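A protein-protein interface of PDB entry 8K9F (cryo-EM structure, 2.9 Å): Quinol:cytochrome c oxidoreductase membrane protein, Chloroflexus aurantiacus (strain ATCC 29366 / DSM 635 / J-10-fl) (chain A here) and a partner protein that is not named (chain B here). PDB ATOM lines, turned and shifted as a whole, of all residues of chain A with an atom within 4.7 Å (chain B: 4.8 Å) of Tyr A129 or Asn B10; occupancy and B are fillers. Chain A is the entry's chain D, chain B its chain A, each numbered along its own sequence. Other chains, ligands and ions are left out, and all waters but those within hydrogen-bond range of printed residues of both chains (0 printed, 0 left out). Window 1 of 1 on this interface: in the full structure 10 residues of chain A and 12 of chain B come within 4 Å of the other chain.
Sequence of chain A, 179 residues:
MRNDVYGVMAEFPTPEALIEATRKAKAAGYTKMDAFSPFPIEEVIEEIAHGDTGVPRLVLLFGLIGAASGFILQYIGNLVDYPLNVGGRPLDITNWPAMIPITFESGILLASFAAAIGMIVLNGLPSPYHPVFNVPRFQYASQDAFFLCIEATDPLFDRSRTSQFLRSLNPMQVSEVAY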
ATOM      1  N   SER A 127      23.285 -17.332  23.070  1.00  0.00           N
ATOM      2  CA  SER A 127      24.344 -17.153  24.059  1.00  0.00           C
ATOM      3  C   SER A 127      25.193 -15.981  23.602  1.00  0.00           C
ATOM      4  O   SER A 127      26.144 -16.158  22.824  1.00  0.00           O
ATOM      5  CB  SER A 127      25.189 -18.414  24.216  1.00  0.00           C
ATOM      6  OG  SER A 127      26.252 -18.210  25.124  1.00  0.00           O
ATOM      7  N   PRO A 128      24.860 -14.758  24.031  1.00  0.00           N
ATOM      8  CA  PRO A 128      25.657 -13.593  23.615  1.00  0.00           C
ATOM      9  C   PRO A 128      27.066 -13.589  24.172  1.00  0.00           C
ATOM     10  O   PRO A 128      27.959 -13.002  23.548  1.00  0.00           O
ATOM     11  CB  PRO A 128      24.853 -12.392  24.133  1.00  0.00           C
ATOM     12  CG  PRO A 128      23.592 -12.919  24.683  1.00  0.00           C
ATOM     13  CD  PRO A 128      23.663 -14.396  24.802  1.00  0.00           C
ATOM     14  N   TYR A 129      27.296 -14.225  25.317  1.00  0.00           N
ATOM     15  CA  TYR A 129      28.620 -14.323  25.913  1.00  0.00           C
ATOM     16  C   TYR A 129      29.145 -15.744  25.769  1.00  0.00           C
ATOM     17  O   TYR A 129      28.494 -16.698  26.203  1.00  0.00           O
ATOM     18  CB  TYR A 129      28.591 -13.928  27.391  1.00  0.00           C
ATOM     19  CG  TYR A 129      29.735 -14.511  28.203  1.00  0.00           C
ATOM     20  CD1 TYR A 129      31.025 -14.016  28.077  1.00  0.00           C
ATOM     21  CD2 TYR A 129      29.520 -15.557  29.099  1.00  0.00           C
ATOM     22  CE1 TYR A 129      32.069 -14.549  28.807  1.00  0.00           C
ATOM     23  CE2 TYR A 129      30.557 -16.095  29.826  1.00  0.00           C
ATOM     24  CZ  TYR A 129      31.830 -15.586  29.680  1.00  0.00           C
ATOM     25  OH  TYR A 129      32.871 -16.113  30.413  1.00  0.00           O
ATOM     26  N   HIS A 130      30.325 -15.875  25.177  1.00  0.00           N
ATOM     27  CA  HIS A 130      31.049 -17.133  25.115  1.00  0.00           C
ATOM     28  C   HIS A 130      32.503 -16.815  25.416  1.00  0.00           C
ATOM     29  O   HIS A 130      32.947 -15.689  25.163  1.00  0.00           O
ATOM     30  CB  HIS A 130      30.913 -17.808  23.737  1.00  0.00           C
ATOM     31  CG  HIS A 130      31.420 -19.216  23.701  1.00  0.00           C
ATOM     32  ND1 HIS A 130      32.740 -19.529  23.477  1.00  0.00           N
ATOM     33  CD2 HIS A 130      30.797 -20.390  23.957  1.00  0.00           C
ATOM     34  CE1 HIS A 130      32.898 -20.840  23.529  1.00  0.00           C
ATOM     35  NE2 HIS A 130      31.732 -21.386  23.819  1.00  0.00           N
ATOM     36  N   PRO A 131      33.245 -17.756  26.017  1.00  0.00           N
ATOM     37  CA  PRO A 131      34.669 -17.506  26.301  1.00  0.00           C
ATOM     38  C   PRO A 131      35.512 -17.174  25.086  1.00  0.00           C
ATOM     39  O   PRO A 131      36.392 -16.316  25.184  1.00  0.00           O
ATOM     40  CB  PRO A 131      35.119 -18.826  26.934  1.00  0.00           C
ATOM     41  CG  PRO A 131      33.932 -19.294  27.647  1.00  0.00           C
ATOM     42  CD  PRO A 131      32.734 -18.869  26.837  1.00  0.00           C
ATOM     43  N   TYR A 179      38.276 -18.138  30.310  1.00  0.00           N
ATOM     44  CA  TYR A 179      36.916 -18.648  30.440  1.00  0.00           C
ATOM     45  C   TYR A 179      35.861 -17.568  30.198  1.00  0.00           C
ATOM     46  O   TYR A 179      36.115 -16.561  29.537  1.00  0.00           O
ATOM     47  CB  TYR A 179      36.718 -19.267  31.822  1.00  0.00           C
ATOM     48  CG  TYR A 179      35.707 -20.386  31.860  1.00  0.00           C
ATOM     49  CD1 TYR A 179      35.769 -21.439  30.955  1.00  0.00           C
ATOM     50  CD2 TYR A 179      34.686 -20.386  32.801  1.00  0.00           C
ATOM     51  CE1 TYR A 179      34.839 -22.466  30.993  1.00  0.00           C
ATOM     52  CE2 TYR A 179      33.751 -21.405  32.846  1.00  0.00           C
ATOM     53  CZ  TYR A 179      33.832 -22.442  31.941  1.00  0.00           C
ATOM     54  OH  TYR A 179      32.903 -23.453  31.991  1.00  0.00           O
ATOM     55  N   ALA B   2      32.148 -12.181  25.275  1.00  0.00           N
ATOM     56  CA  ALA B   2      32.776 -11.316  26.265  1.00  0.00           C
ATOM     57  C   ALA B   2      33.343 -10.069  25.611  1.00  0.00           C
ATOM     58  O   ALA B   2      33.662  -9.092  26.287  1.00  0.00           O
ATOM     59  CB  ALA B   2      33.861 -12.055  26.994  1.00  0.00           C
ATOM     60  N   PHE B   5      29.502  -8.263  25.151  1.00  0.00           N
ATOM     61  CA  PHE B   5      28.510  -8.503  26.181  1.00  0.00           C
ATOM     62  C   PHE B   5      29.177  -8.873  27.504  1.00  0.00           C
ATOM     63  O   PHE B   5      30.296  -9.389  27.507  1.00  0.00           O
ATOM     64  CB  PHE B   5      27.606  -9.647  25.703  1.00  0.00           C
ATOM     65  CG  PHE B   5      26.704  -9.274  24.560  1.00  0.00           C
ATOM     66  CD1 PHE B   5      25.521  -8.586  24.781  1.00  0.00           C
ATOM     67  CD2 PHE B   5      27.043  -9.614  23.263  1.00  0.00           C
ATOM     68  CE1 PHE B   5      24.693  -8.249  23.727  1.00  0.00           C
ATOM     69  CE2 PHE B   5      26.221  -9.277  22.206  1.00  0.00           C
ATOM     70  CZ  PHE B   5      25.046  -8.595  22.439  1.00  0.00           C
ATOM     71  N   PRO B   6      28.434  -8.713  28.662  1.00  0.00           N
ATOM     72  CA  PRO B   6      29.128  -9.074  29.893  1.00  0.00           C
ATOM     73  C   PRO B   6      29.020 -10.547  30.241  1.00  0.00           C
ATOM     74  O   PRO B   6      28.672 -11.340  29.395  1.00  0.00           O
ATOM     75  CB  PRO B   6      28.348  -8.325  30.976  1.00  0.00           C
ATOM     76  CG  PRO B   6      27.171  -7.697  30.330  1.00  0.00           C
ATOM     77  CD  PRO B   6      27.034  -8.338  29.001  1.00  0.00           C
ATOM     78  N   ARG B   7      29.311 -10.909  31.488  1.00  0.00           N
ATOM     79  CA  ARG B   7      29.309 -12.326  31.836  1.00  0.00           C
ATOM     80  C   ARG B   7      27.910 -12.924  31.940  1.00  0.00           C
ATOM     81  O   ARG B   7      27.680 -14.052  31.487  1.00  0.00           O
ATOM     82  CB  ARG B   7      30.077 -12.539  33.138  1.00  0.00           C
ATOM     83  CG  ARG B   7      30.452 -13.993  33.374  1.00  0.00           C
ATOM     84  CD  ARG B   7      31.185 -14.194  34.686  1.00  0.00           C
ATOM     85  NE  ARG B   7      32.156 -15.277  34.586  1.00  0.00           N
ATOM     86  CZ  ARG B   7      33.436 -15.113  34.289  1.00  0.00           C
ATOM     87  NH1 ARG B   7      33.958 -13.911  34.121  1.00  0.00           N
ATOM     88  NH2 ARG B   7      34.214 -16.182  34.159  1.00  0.00           N
ATOM     89  N   ASN B   8      26.958 -12.190  32.519  1.00  0.00           N
ATOM     90  CA  ASN B   8      25.595 -12.679  32.667  1.00  0.00           C
ATOM     91  C   ASN B   8      24.703 -12.319  31.484  1.00  0.00           C
ATOM     92  O   ASN B   8      23.475 -12.257  31.638  1.00  0.00           O
ATOM     93  CB  ASN B   8      24.989 -12.175  33.982  1.00  0.00           C
ATOM     94  CG  ASN B   8      25.267 -10.702  34.241  1.00  0.00           C
ATOM     95  OD1 ASN B   8      25.231  -9.872  33.330  1.00  0.00           O
ATOM     96  ND2 ASN B   8      25.555 -10.375  35.496  1.00  0.00           N
ATOM     97  N   ALA B   9      25.292 -12.089  30.307  1.00  0.00           N
ATOM     98  CA  ALA B   9      24.503 -11.906  29.094  1.00  0.00           C
ATOM     99  C   ALA B   9      23.752 -13.170  28.720  1.00  0.00           C
ATOM    100  O   ALA B   9      22.623 -13.090  28.226  1.00  0.00           O
ATOM    101  CB  ALA B   9      25.395 -11.494  27.938  1.00  0.00           C
ATOM    102  N   ASN B  10      24.368 -14.334  28.938  1.00  0.00           N
ATOM    103  CA  ASN B  10      23.682 -15.604  28.738  1.00  0.00           C
ATOM    104  C   ASN B  10      22.479 -15.733  29.663  1.00  0.00           C
ATOM    105  O   ASN B  10      21.393 -16.144  29.230  1.00  0.00           O
ATOM    106  CB  ASN B  10      24.668 -16.749  28.955  1.00  0.00           C
ATOM    107  CG  ASN B  10      25.773 -16.760  27.923  1.00  0.00           C
ATOM    108  OD1 ASN B  10      25.751 -15.977  26.978  1.00  0.00           O
ATOM    109  ND2 ASN B  10      26.755 -17.636  28.104  1.00  0.00           N
ATOM    110  N   LEU B  11      22.653 -15.341  30.930  1.00  0.00           N
ATOM    111  CA  LEU B  11      21.564 -15.348  31.902  1.00  0.00           C
ATOM    112  C   LEU B  11      20.425 -14.435  31.470  1.00  0.00           C
ATOM    113  O   LEU B  11      19.259 -14.848  31.432  1.00  0.00           O
ATOM    114  CB  LEU B  11      22.106 -14.910  33.258  1.00  0.00           C
ATOM    115  CG  LEU B  11      21.608 -15.542  34.551  1.00  0.00           C
ATOM    116  CD1 LEU B  11      21.187 -16.967  34.327  1.00  0.00           C
ATOM    117  CD2 LEU B  11      22.721 -15.469  35.584  1.00  0.00           C
ATOM    118  N   LEU B  12      20.762 -13.198  31.093  1.00  0.00           N
ATOM    119  CA  LEU B  12      19.750 -12.217  30.725  1.00  0.00           C
ATOM    120  C   LEU B  12      19.059 -12.578  29.421  1.00  0.00           C
ATOM    121  O   LEU B  12      17.863 -12.320  29.273  1.00  0.00           O
ATOM    122  CB  LEU B  12      20.370 -10.823  30.630  1.00  0.00           C
ATOM    123  CG  LEU B  12      20.357  -9.908  31.858  1.00  0.00           C
ATOM    124  CD1 LEU B  12      20.966 -10.553  33.112  1.00  0.00           C
ATOM    125  CD2 LEU B  12      21.054  -8.595  31.531  1.00  0.00           C
ATOM    126  N   SER B  13      19.770 -13.215  28.488  1.00  0.00           N
ATOM    127  CA  SER B  13      19.158 -13.598  27.221  1.00  0.00           C
ATOM    128  C   SER B  13      18.216 -14.785  27.387  1.00  0.00           C
ATOM    129  O   SER B  13      17.121 -14.797  26.809  1.00  0.00           O
ATOM    130  CB  SER B  13      20.244 -13.904  26.192  1.00  0.00           C
ATOM    131  OG  SER B  13      20.893 -15.127  26.489  1.00  0.00           O
ATOM    132  N   ARG B  14      18.631 -15.807  28.152  1.00  0.00           N
ATOM    133  CA  ARG B  14      17.731 -16.926  28.440  1.00  0.00           C
ATOM    134  C   ARG B  14      16.499 -16.457  29.202  1.00  0.00           C
ATOM    135  O   ARG B  14      15.366 -16.834  28.863  1.00  0.00           O
ATOM    136  CB  ARG B  14      18.452 -18.018  29.230  1.00  0.00           C
ATOM    137  CG  ARG B  14      19.136 -19.121  28.414  1.00  0.00           C
ATOM    138  CD  ARG B  14      20.297 -18.661  27.551  1.00  0.00           C
ATOM    139  NE  ARG B  14      20.993 -19.796  26.958  1.00  0.00           N
ATOM    140  CZ  ARG B  14      22.287 -19.814  26.668  1.00  0.00           C
ATOM    141  NH1 ARG B  14      23.048 -18.751  26.847  1.00  0.00           N
ATOM    142  NH2 ARG B  14      22.828 -20.926  26.181  1.00  0.00           N
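OD1 of Asn B10 lies within hydrogen-bond range of OG of Ser A127 (2.9 Å). ND2 of Asn B10 lies within hydrogen-bond range of O of Tyr A129. The backbone nitrogen (N) of Pro A128 sits close to the side-chain amide oxygen (OD1) of Asn B10 (3.3 Å).
The backbone carbonyl oxygen of Ala B9 sits at hydrogen-bond distance from the side-chain hydroxyl of Ser B13 (3.2 Å). O of Asn B10 sits at hydrogen-bond distance from OG of Ser B13 (3.0 Å). O of Tyr A129 sits at hydrogen-bond distance from OG of Ser A127 (2.9 Å). The side-chain hydroxyl (OH) of Tyr A129 lies close to the backbone carbonyl oxygen (O) of Tyr A179.
Ser A127 touches Arg B14. O of Pro A128 touches CD2 of Phe B5 (3.5 Å). Pro A128 touches Ala B9. Pro A128 touches Ser B13 (CD to OG, 3.3 Å). Tyr A129 touches Ala B2. Pro B6 touches Tyr A129 (O to CB, 3.3 Å). Arg B7 touches Tyr A129. His A130 touches Ala B2.
Of the printed residues of chain B, Ser A127 touches Asn B10 and Arg B14. Printed residues of chain B within 4 Å of Pro A128: Phe B5, Ala B9, Asn B10 and Ser B13. Of chain B, only Ala B2 (3.5 Å), Pro B6 (3.3 Å), Arg B7 (3.4 Å) and Asn B10 (2.7 Å) come within 4 Å of Tyr A129. Printed residues of chain A within 4 Å of Pro B6: Tyr A129 (3.3 Å). Of the printed residues of chain A, Arg B7 touches Tyr A129 (3.4 Å). Printed residues of chain A within 4 Å of Asn B10: Ser A127 (2.9 Å), Pro A128 (3.3 Å) and Tyr A129 (2.7 Å). Printed residues of chain A within 4 Å of Ser B13: Pro A128 (3.3 Å). The nearest printed residue of chain A that does not touch Asn B10 is His A130 (4.9 Å).
Of the 11 printed residues of chain B, 8 touch a printed residue of chain A. Of the 6 printed residues of chain A, 4 touch a printed residue of chain B. Among the printed residues, no Asp or Glu carboxylate lies within 4 Å of a Lys or Arg side-chain nitrogen of the other chain.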
